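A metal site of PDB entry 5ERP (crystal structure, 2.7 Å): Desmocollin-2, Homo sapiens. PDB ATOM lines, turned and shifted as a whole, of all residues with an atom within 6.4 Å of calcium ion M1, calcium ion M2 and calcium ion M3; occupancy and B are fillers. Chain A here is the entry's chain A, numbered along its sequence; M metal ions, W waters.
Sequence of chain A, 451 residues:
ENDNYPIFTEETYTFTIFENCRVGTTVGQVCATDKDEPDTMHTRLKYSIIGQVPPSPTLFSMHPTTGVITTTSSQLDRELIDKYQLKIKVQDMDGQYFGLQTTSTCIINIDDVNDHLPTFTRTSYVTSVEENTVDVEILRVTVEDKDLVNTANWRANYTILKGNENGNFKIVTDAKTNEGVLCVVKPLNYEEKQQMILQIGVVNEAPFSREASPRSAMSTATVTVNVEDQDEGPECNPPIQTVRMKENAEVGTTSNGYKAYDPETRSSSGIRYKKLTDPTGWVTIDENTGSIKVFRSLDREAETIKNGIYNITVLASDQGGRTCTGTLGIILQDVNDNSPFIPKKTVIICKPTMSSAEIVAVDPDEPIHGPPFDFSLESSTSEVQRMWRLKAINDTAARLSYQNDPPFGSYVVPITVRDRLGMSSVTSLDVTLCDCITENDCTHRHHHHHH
Calcium ion M1 is bound by O of His 116 (2.3 Å), OD2 of Asp 147 (2.3 Å), O of Asn 153 (2.3 Å), OD1 of Asn 114 (2.4 Å), OD2 of Asp 145 (2.5 Å), OD1 of Asp 145 (2.7 Å) and OD1 of Asn 204 (2.8 Å).
Calcium ion M1 has seven donor atoms within binding distance.
The backbone NH (N) of Arg 78 sits close to the side-chain carboxylate (OE1) of Glu 19 (3.2 Å).
The backbone carbonyl oxygen (O) of Asp 111 lies within hydrogen-bond range of the backbone NH (N) of Glu 19 (3.4 Å).
The side-chain carboxylate (OD1) of Asp 115 lies close to a ring nitrogen (ND1) of His 116 (3.3 Å).
ND2 of Asn 153 sits at hydrogen-bond distance from OD2 of Asp 112, at 3.2 Å.
The side-chain carboxylate of Asp 112 sits close to the guanidinium group of Arg 78, at 3.1 Å.
The side-chain amide nitrogen (ND2) of Asn 204 sits at hydrogen-bond distance from the backbone carbonyl oxygen (O) of Trp 154.
ND2 of Asn 114 lies close to N of Phe 208, 3.4 Å away.
The backbone NH (N) of Leu 148 lies within hydrogen-bond range of the side-chain carboxylate (OD2) of Asp 112, at 3.2 Å.
Calcium ion M2 is bound by the side-chain carboxylate of Glu 79 (2.3 Å), the side-chain carboxylate of Asp 115 (2.4 Å), the side-chain carboxylate of Asp 112 (2.4 Å), the side-chain carboxylate of Glu 19 (2.5 Å), the side-chain carboxylate of Asp 147 (2.5 Å) and the backbone carbonyl oxygen of Val 113 (2.6 Å).
Within 4 Å of calcium ion M1: Asn 114, His 116, Asp 145, Asp 147, Asn 153 and Asn 204.
The nearest printed residue that does not touch calcium ion M1 is Pro 118 (4.4 Å).
Six residues have an atom within 4 Å of calcium ion M2: Glu 19, Glu 79, Asp 112, Val 113, Asp 115 and Asp 147.
Within 4 Å of calcium ion M3: Glu 19, Asp 77, Glu 79 and Asp 115.
Calcium ion M3 is bound by the side-chain carboxylate of Asp 77 (2.3 Å), the side-chain carboxylate of Asp 115 (2.3 Å), water W1 (2.4 Å), the side-chain carboxylate of Glu 79 (2.4 Å), water W2 (2.5 Å) and the side-chain carboxylate of Glu 19 (2.5 Å).
Calcium ion M3 has six donor atoms within binding distance.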
ATOM      1  N   GLU A  19      15.831 -16.519  -0.038  1.00  0.00           N
ATOM      2  CA  GLU A  19      15.809 -17.682  -0.915  1.00  0.00           C
ATOM      3  C   GLU A  19      14.669 -17.554  -1.925  1.00  0.00           C
ATOM      4  O   GLU A  19      13.716 -16.796  -1.701  1.00  0.00           O
ATOM      5  CB  GLU A  19      15.663 -18.969  -0.100  1.00  0.00           C
ATOM      6  CG  GLU A  19      14.374 -19.033   0.708  1.00  0.00           C
ATOM      7  CD  GLU A  19      14.231 -20.342   1.461  1.00  0.00           C
ATOM      8  OE1 GLU A  19      14.664 -21.396   0.941  1.00  0.00           O
ATOM      9  OE2 GLU A  19      13.684 -20.314   2.576  1.00  0.00           O
ATOM     10  N   ASN A  20      14.770 -18.304  -3.012  1.00  0.00           N
ATOM     11  CA  ASN A  20      13.757 -18.306  -4.061  1.00  0.00           C
ATOM     12  C   ASN A  20      13.583 -16.945  -4.738  1.00  0.00           C
ATOM     13  O   ASN A  20      12.597 -16.722  -5.443  1.00  0.00           O
ATOM     14  CB  ASN A  20      12.414 -18.778  -3.510  1.00  0.00           C
ATOM     15  CG  ASN A  20      12.518 -20.078  -2.749  1.00  0.00           C
ATOM     16  OD1 ASN A  20      13.429 -20.872  -3.001  1.00  0.00           O
ATOM     17  ND2 ASN A  20      11.584 -20.318  -1.832  1.00  0.00           N
ATOM     18  N   LEU A  76      18.263 -20.666  -5.238  1.00  0.00           N
ATOM     19  CA  LEU A  76      18.863 -20.488  -3.922  1.00  0.00           C
ATOM     20  C   LEU A  76      17.927 -21.092  -2.875  1.00  0.00           C
ATOM     21  O   LEU A  76      16.766 -20.704  -2.783  1.00  0.00           O
ATOM     22  CB  LEU A  76      19.104 -19.007  -3.642  1.00  0.00           C
ATOM     23  CG  LEU A  76      20.093 -18.313  -4.577  1.00  0.00           C
ATOM     24  CD1 LEU A  76      19.728 -16.845  -4.737  1.00  0.00           C
ATOM     25  CD2 LEU A  76      21.517 -18.484  -4.060  1.00  0.00           C
ATOM     26  N   ASP A  77      18.454 -22.027  -2.094  1.00  0.00           N
ATOM     27  CA  ASP A  77      17.641 -22.778  -1.146  1.00  0.00           C
ATOM     28  C   ASP A  77      18.315 -22.851   0.216  1.00  0.00           C
ATOM     29  O   ASP A  77      19.358 -23.497   0.368  1.00  0.00           O
ATOM     30  CB  ASP A  77      17.362 -24.182  -1.681  1.00  0.00           C
ATOM     31  CG  ASP A  77      16.272 -24.902  -0.904  1.00  0.00           C
ATOM     32  OD1 ASP A  77      15.601 -24.264  -0.076  1.00  0.00           O
ATOM     33  OD2 ASP A  77      16.082 -26.117  -1.130  1.00  0.00           O
ATOM     34  N   ARG A  78      17.720 -22.188   1.195  1.00  0.00           N
ATOM     35  CA  ARG A  78      18.289 -22.074   2.528  1.00  0.00           C
ATOM     36  C   ARG A  78      18.431 -23.442   3.192  1.00  0.00           C
ATOM     37  O   ARG A  78      19.363 -23.672   3.962  1.00  0.00           O
ATOM     38  CB  ARG A  78      17.408 -21.161   3.401  1.00  0.00           C
ATOM     39  CG  ARG A  78      18.145 -20.556   4.593  1.00  0.00           C
ATOM     40  CD  ARG A  78      17.262 -20.390   5.833  1.00  0.00           C
ATOM     41  NE  ARG A  78      17.523 -21.423   6.825  1.00  0.00           N
ATOM     42  CZ  ARG A  78      16.754 -22.487   7.057  1.00  0.00           C
ATOM     43  NH1 ARG A  78      15.626 -22.670   6.384  1.00  0.00           N
ATOM     44  NH2 ARG A  78      17.127 -23.352   7.981  1.00  0.00           N
ATOM     45  N   GLU A  79      17.506 -24.348   2.884  1.00  0.00           N
ATOM     46  CA  GLU A  79      17.485 -25.677   3.493  1.00  0.00           C
ATOM     47  C   GLU A  79      18.539 -26.613   2.902  1.00  0.00           C
ATOM     48  O   GLU A  79      18.777 -27.695   3.425  1.00  0.00           O
ATOM     49  CB  GLU A  79      16.087 -26.292   3.354  1.00  0.00           C
ATOM     50  CG  GLU A  79      15.044 -25.673   4.289  1.00  0.00           C
ATOM     51  CD  GLU A  79      14.505 -24.340   3.796  1.00  0.00           C
ATOM     52  OE1 GLU A  79      14.635 -24.042   2.589  1.00  0.00           O
ATOM     53  OE2 GLU A  79      13.952 -23.581   4.625  1.00  0.00           O
ATOM     54  N   LEU A  80      19.157 -26.192   1.793  1.00  0.00           N
ATOM     55  CA  LEU A  80      20.252 -26.965   1.184  1.00  0.00           C
ATOM     56  C   LEU A  80      21.590 -26.291   1.476  1.00  0.00           C
ATOM     57  O   LEU A  80      22.522 -26.936   1.952  1.00  0.00           O
ATOM     58  CB  LEU A  80      20.047 -27.099  -0.324  1.00  0.00           C
ATOM     59  CG  LEU A  80      18.852 -27.953  -0.781  1.00  0.00           C
ATOM     60  CD1 LEU A  80      18.663 -27.852  -2.287  1.00  0.00           C
ATOM     61  CD2 LEU A  80      19.044 -29.405  -0.367  1.00  0.00           C
ATOM     62  N   ASP A 111      18.468 -15.716   3.671  1.00  0.00           N
ATOM     63  CA  ASP A 111      17.433 -15.528   4.660  1.00  0.00           C
ATOM     64  C   ASP A 111      16.298 -16.502   4.382  1.00  0.00           C
ATOM     65  O   ASP A 111      16.160 -17.006   3.264  1.00  0.00           O
ATOM     66  CB  ASP A 111      16.929 -14.088   4.639  1.00  0.00           C
ATOM     67  CG  ASP A 111      16.528 -13.575   6.007  1.00  0.00           C
ATOM     68  OD1 ASP A 111      16.065 -14.383   6.840  1.00  0.00           O
ATOM     69  OD2 ASP A 111      16.670 -12.365   6.245  1.00  0.00           O
ATOM     70  N   ASP A 112      15.472 -16.771   5.392  1.00  0.00           N
ATOM     71  CA  ASP A 112      14.432 -17.779   5.283  1.00  0.00           C
ATOM     72  C   ASP A 112      13.088 -17.184   4.848  1.00  0.00           C
ATOM     73  O   ASP A 112      12.742 -16.066   5.225  1.00  0.00           O
ATOM     74  CB  ASP A 112      14.261 -18.508   6.618  1.00  0.00           C
ATOM     75  CG  ASP A 112      13.304 -19.681   6.538  1.00  0.00           C
ATOM     76  OD1 ASP A 112      13.526 -20.558   5.679  1.00  0.00           O
ATOM     77  OD2 ASP A 112      12.340 -19.717   7.334  1.00  0.00           O
ATOM     78  N   VAL A 113      12.359 -17.947   4.037  1.00  0.00           N
ATOM     79  CA  VAL A 113      10.957 -17.653   3.738  1.00  0.00           C
ATOM     80  C   VAL A 113      10.158 -18.907   4.035  1.00  0.00           C
ATOM     81  O   VAL A 113      10.712 -20.011   4.051  1.00  0.00           O
ATOM     82  CB  VAL A 113      10.738 -17.192   2.272  1.00  0.00           C
ATOM     83  CG1 VAL A 113      11.715 -16.083   1.892  1.00  0.00           C
ATOM     84  CG2 VAL A 113      10.865 -18.362   1.310  1.00  0.00           C
ATOM     85  N   ASN A 114       8.859 -18.757   4.276  1.00  0.00           N
ATOM     86  CA  ASN A 114       8.012 -19.874   4.664  1.00  0.00           C
ATOM     87  C   ASN A 114       7.579 -20.714   3.457  1.00  0.00           C
ATOM     88  O   ASN A 114       6.520 -20.458   2.878  1.00  0.00           O
ATOM     89  CB  ASN A 114       6.781 -19.357   5.420  1.00  0.00           C
ATOM     90  CG  ASN A 114       5.874 -20.474   5.920  1.00  0.00           C
ATOM     91  OD1 ASN A 114       6.335 -21.553   6.272  1.00  0.00           O
ATOM     92  ND2 ASN A 114       4.585 -20.196   5.964  1.00  0.00           N
ATOM     93  N   ASP A 115       8.394 -21.688   3.083  1.00  0.00           N
ATOM     94  CA  ASP A 115       8.103 -22.532   1.917  1.00  0.00           C
ATOM     95  C   ASP A 115       8.006 -24.014   2.268  1.00  0.00           C
ATOM     96  O   ASP A 115       7.943 -24.863   1.370  1.00  0.00           O
ATOM     97  CB  ASP A 115       9.160 -22.316   0.825  1.00  0.00           C
ATOM     98  CG  ASP A 115      10.582 -22.504   1.327  1.00  0.00           C
ATOM     99  OD1 ASP A 115      10.777 -22.716   2.534  1.00  0.00           O
ATOM    100  OD2 ASP A 115      11.496 -22.427   0.489  1.00  0.00           O
ATOM    101  N   HIS A 116       8.001 -24.328   3.557  1.00  0.00           N
ATOM    102  CA  HIS A 116       7.619 -25.666   4.035  1.00  0.00           C
ATOM    103  C   HIS A 116       6.438 -25.562   4.983  1.00  0.00           C
ATOM    104  O   HIS A 116       6.528 -24.938   6.036  1.00  0.00           O
ATOM    105  CB  HIS A 116       8.791 -26.358   4.743  1.00  0.00           C
ATOM    106  CG  HIS A 116       9.941 -26.693   3.849  1.00  0.00           C
ATOM    107  ND1 HIS A 116      11.007 -25.841   3.650  1.00  0.00           N
ATOM    108  CD2 HIS A 116      10.201 -27.801   3.114  1.00  0.00           C
ATOM    109  CE1 HIS A 116      11.864 -26.405   2.822  1.00  0.00           C
ATOM    110  NE2 HIS A 116      11.398 -27.595   2.475  1.00  0.00           N
ATOM    111  N   LEU A 117       5.314 -26.182   4.623  1.00  0.00           N
ATOM    112  CA  LEU A 117       4.152 -26.190   5.497  1.00  0.00           C
ATOM    113  C   LEU A 117       4.385 -27.166   6.633  1.00  0.00           C
ATOM    114  O   LEU A 117       4.964 -28.242   6.417  1.00  0.00           O
ATOM    115  CB  LEU A 117       2.882 -26.567   4.735  1.00  0.00           C
ATOM    116  CG  LEU A 117       2.485 -25.612   3.611  1.00  0.00           C
ATOM    117  CD1 LEU A 117       1.510 -26.287   2.661  1.00  0.00           C
ATOM    118  CD2 LEU A 117       1.845 -24.356   4.206  1.00  0.00           C
ATOM    119  N   PRO A 118       3.945 -26.827   7.857  1.00  0.00           N
ATOM    120  CA  PRO A 118       4.157 -27.760   8.959  1.00  0.00           C
ATOM    121  C   PRO A 118       3.187 -28.928   8.869  1.00  0.00           C
ATOM    122  O   PRO A 118       2.035 -28.754   8.484  1.00  0.00           O
ATOM    123  CB  PRO A 118       3.900 -26.906  10.194  1.00  0.00           C
ATOM    124  CG  PRO A 118       2.891 -25.908   9.740  1.00  0.00           C
ATOM    125  CD  PRO A 118       3.167 -25.651   8.276  1.00  0.00           C
ATOM    126  N   ASP A 145       8.697 -29.132  10.501  1.00  0.00           N
ATOM    127  CA  ASP A 145       8.793 -27.921   9.700  1.00  0.00           C
ATOM    128  C   ASP A 145      10.260 -27.649   9.407  1.00  0.00           C
ATOM    129  O   ASP A 145      11.055 -27.452  10.326  1.00  0.00           O
ATOM    130  CB  ASP A 145       8.153 -26.731  10.414  1.00  0.00           C
ATOM    131  CG  ASP A 145       7.862 -25.573   9.478  1.00  0.00           C
ATOM    132  OD1 ASP A 145       8.734 -25.227   8.662  1.00  0.00           O
ATOM    133  OD2 ASP A 145       6.751 -25.011   9.565  1.00  0.00           O
ATOM    134  N   LYS A 146      10.601 -27.628   8.124  1.00  0.00           N
ATOM    135  CA  LYS A 146      11.992 -27.524   7.711  1.00  0.00           C
ATOM    136  C   LYS A 146      12.480 -26.081   7.634  1.00  0.00           C
ATOM    137  O   LYS A 146      13.651 -25.838   7.330  1.00  0.00           O
ATOM    138  CB  LYS A 146      12.176 -28.215   6.364  1.00  0.00           C
ATOM    139  CG  LYS A 146      12.203 -29.724   6.480  1.00  0.00           C
ATOM    140  CD  LYS A 146      11.916 -30.417   5.165  1.00  0.00           C
ATOM    141  CE  LYS A 146      11.873 -31.925   5.322  1.00  0.00           C
ATOM    142  NZ  LYS A 146      13.145 -32.454   5.900  1.00  0.00           N
ATOM    143  N   ASP A 147      11.601 -25.133   7.928  1.00  0.00           N
ATOM    144  CA  ASP A 147      11.993 -23.724   7.880  1.00  0.00           C
ATOM    145  C   ASP A 147      12.829 -23.384   9.110  1.00  0.00           C
ATOM    146  O   ASP A 147      13.067 -24.235   9.962  1.00  0.00           O
ATOM    147  CB  ASP A 147      10.759 -22.821   7.789  1.00  0.00           C
ATOM    148  CG  ASP A 147      10.051 -22.947   6.455  1.00  0.00           C
ATOM    149  OD1 ASP A 147      10.737 -23.136   5.428  1.00  0.00           O
ATOM    150  OD2 ASP A 147       8.805 -22.844   6.427  1.00  0.00           O
ATOM    151  N   LEU A 148      13.263 -22.137   9.184  1.00  0.00           N
ATOM    152  CA  LEU A 148      14.229 -21.714  10.187  1.00  0.00           C
ATOM    153  C   LEU A 148      13.622 -21.618  11.589  1.00  0.00           C
ATOM    154  O   LEU A 148      12.620 -20.932  11.790  1.00  0.00           O
ATOM    155  CB  LEU A 148      14.848 -20.381   9.785  1.00  0.00           C
ATOM    156  CG  LEU A 148      15.856 -19.764  10.757  1.00  0.00           C
ATOM    157  CD1 LEU A 148      17.029 -20.699  10.973  1.00  0.00           C
ATOM    158  CD2 LEU A 148      16.323 -18.419  10.235  1.00  0.00           C
ATOM    159  N   ALA A 152       8.478 -16.925  12.582  1.00  0.00           N
ATOM    160  CA  ALA A 152       7.072 -17.031  12.211  1.00  0.00           C
ATOM    161  C   ALA A 152       6.863 -18.002  11.042  1.00  0.00           C
ATOM    162  O   ALA A 152       5.731 -18.385  10.749  1.00  0.00           O
ATOM    163  CB  ALA A 152       6.517 -15.656  11.852  1.00  0.00           C
ATOM    164  N   ASN A 153       7.945 -18.373  10.376  1.00  0.00           N
ATOM    165  CA  ASN A 153       7.884 -19.341   9.285  1.00  0.00           C
ATOM    166  C   ASN A 153       7.948 -20.764   9.810  1.00  0.00           C
ATOM    167  O   ASN A 153       7.773 -21.720   9.051  1.00  0.00           O
ATOM    168  CB  ASN A 153       9.033 -19.112   8.309  1.00  0.00           C
ATOM    169  CG  ASN A 153       9.056 -17.717   7.735  1.00  0.00           C
ATOM    170  OD1 ASN A 153       8.029 -17.042   7.655  1.00  0.00           O
ATOM    171  ND2 ASN A 153      10.245 -17.253   7.350  1.00  0.00           N
ATOM    172  N   TRP A 154       8.189 -20.906  11.107  1.00  0.00           N
ATOM    173  CA  TRP A 154       8.437 -22.207  11.718  1.00  0.00           C
ATOM    174  C   TRP A 154       7.406 -22.586  12.773  1.00  0.00           C
ATOM    175  O   TRP A 154       6.806 -23.667  12.708  1.00  0.00           O
ATOM    176  CB  TRP A 154       9.827 -22.214  12.354  1.00  0.00           C
ATOM    177  CG  TRP A 154      10.157 -23.455  13.110  1.00  0.00           C
ATOM    178  CD1 TRP A 154      10.539 -24.659  12.590  1.00  0.00           C
ATOM    179  CD2 TRP A 154      10.160 -23.619  14.529  1.00  0.00           C
ATOM    180  NE1 TRP A 154      10.775 -25.556  13.594  1.00  0.00           N
ATOM    181  CE2 TRP A 154      10.555 -24.951  14.796  1.00  0.00           C
ATOM    182  CE3 TRP A 154       9.882 -22.771  15.599  1.00  0.00           C
ATOM    183  CZ2 TRP A 154      10.661 -25.448  16.091  1.00  0.00           C
ATOM    184  CZ3 TRP A 154       9.990 -23.261  16.887  1.00  0.00           C
ATOM    185  CH2 TRP A 154      10.378 -24.584  17.120  1.00  0.00           C
ATOM    186  N   ARG A 155       7.197 -21.710  13.747  1.00  0.00           N
ATOM    187  CA  ARG A 155       6.375 -22.037  14.911  1.00  0.00           C
ATOM    188  C   ARG A 155       4.915 -22.241  14.547  1.00  0.00           C
ATOM    189  O   ARG A 155       4.370 -21.544  13.691  1.00  0.00           O
ATOM    190  CB  ARG A 155       6.499 -20.944  15.968  1.00  0.00           C
ATOM    191  CG  ARG A 155       5.959 -19.597  15.558  1.00  0.00           C
ATOM    192  CD  ARG A 155       6.093 -18.594  16.699  1.00  0.00           C
ATOM    193  NE  ARG A 155       6.758 -17.361  16.283  1.00  0.00           N
ATOM    194  CZ  ARG A 155       8.034 -17.080  16.498  1.00  0.00           C
ATOM    195  NH1 ARG A 155       8.832 -17.941  17.131  1.00  0.00           N
ATOM    196  NH2 ARG A 155       8.528 -15.930  16.076  1.00  0.00           N
ATOM    197  N   ASN A 204       1.559 -22.112  10.249  1.00  0.00           N
ATOM    198  CA  ASN A 204       2.550 -21.216  10.854  1.00  0.00           C
ATOM    199  C   ASN A 204       1.893 -19.879  11.174  1.00  0.00           C
ATOM    200  O   ASN A 204       0.781 -19.602  10.728  1.00  0.00           O
ATOM    201  CB  ASN A 204       3.733 -20.995   9.920  1.00  0.00           C
ATOM    202  CG  ASN A 204       4.346 -22.294   9.431  1.00  0.00           C
ATOM    203  OD1 ASN A 204       4.336 -22.575   8.233  1.00  0.00           O
ATOM    204  ND2 ASN A 204       4.895 -23.079  10.345  1.00  0.00           N
ATOM    205  N   PHE A 208       2.030 -19.199   3.997  1.00  0.00           N
ATOM    206  CA  PHE A 208       2.900 -19.938   3.077  1.00  0.00           C
ATOM    207  C   PHE A 208       3.471 -18.943   2.054  1.00  0.00           C
ATOM    208  O   PHE A 208       2.863 -17.886   1.843  1.00  0.00           O
ATOM    209  CB  PHE A 208       2.102 -21.046   2.371  1.00  0.00           C
ATOM    210  CG  PHE A 208       2.935 -22.060   1.643  1.00  0.00           C
ATOM    211  CD1 PHE A 208       4.091 -22.581   2.216  1.00  0.00           C
ATOM    212  CD2 PHE A 208       2.568 -22.510   0.386  1.00  0.00           C
ATOM    213  CE1 PHE A 208       4.846 -23.533   1.544  1.00  0.00           C
ATOM    214  CE2 PHE A 208       3.330 -23.450  -0.287  1.00  0.00           C
ATOM    215  CZ  PHE A 208       4.469 -23.961   0.292  1.00  0.00           C
HETATM  216 CA    CA M   1       6.942 -23.434   7.698  1.00  0.00          CA
HETATM  217 CA    CA M   2      12.419 -21.917   4.027  1.00  0.00          CA
HETATM  218 CA    CA M   3      13.521 -23.549   0.523  1.00  0.00          CA
HETATM  219  O   HOH W   1      13.608 -22.790  -1.720  1.00  0.00           O
HETATM  220  O   HOH W   2      12.660 -25.793   0.028  1.00  0.00           O
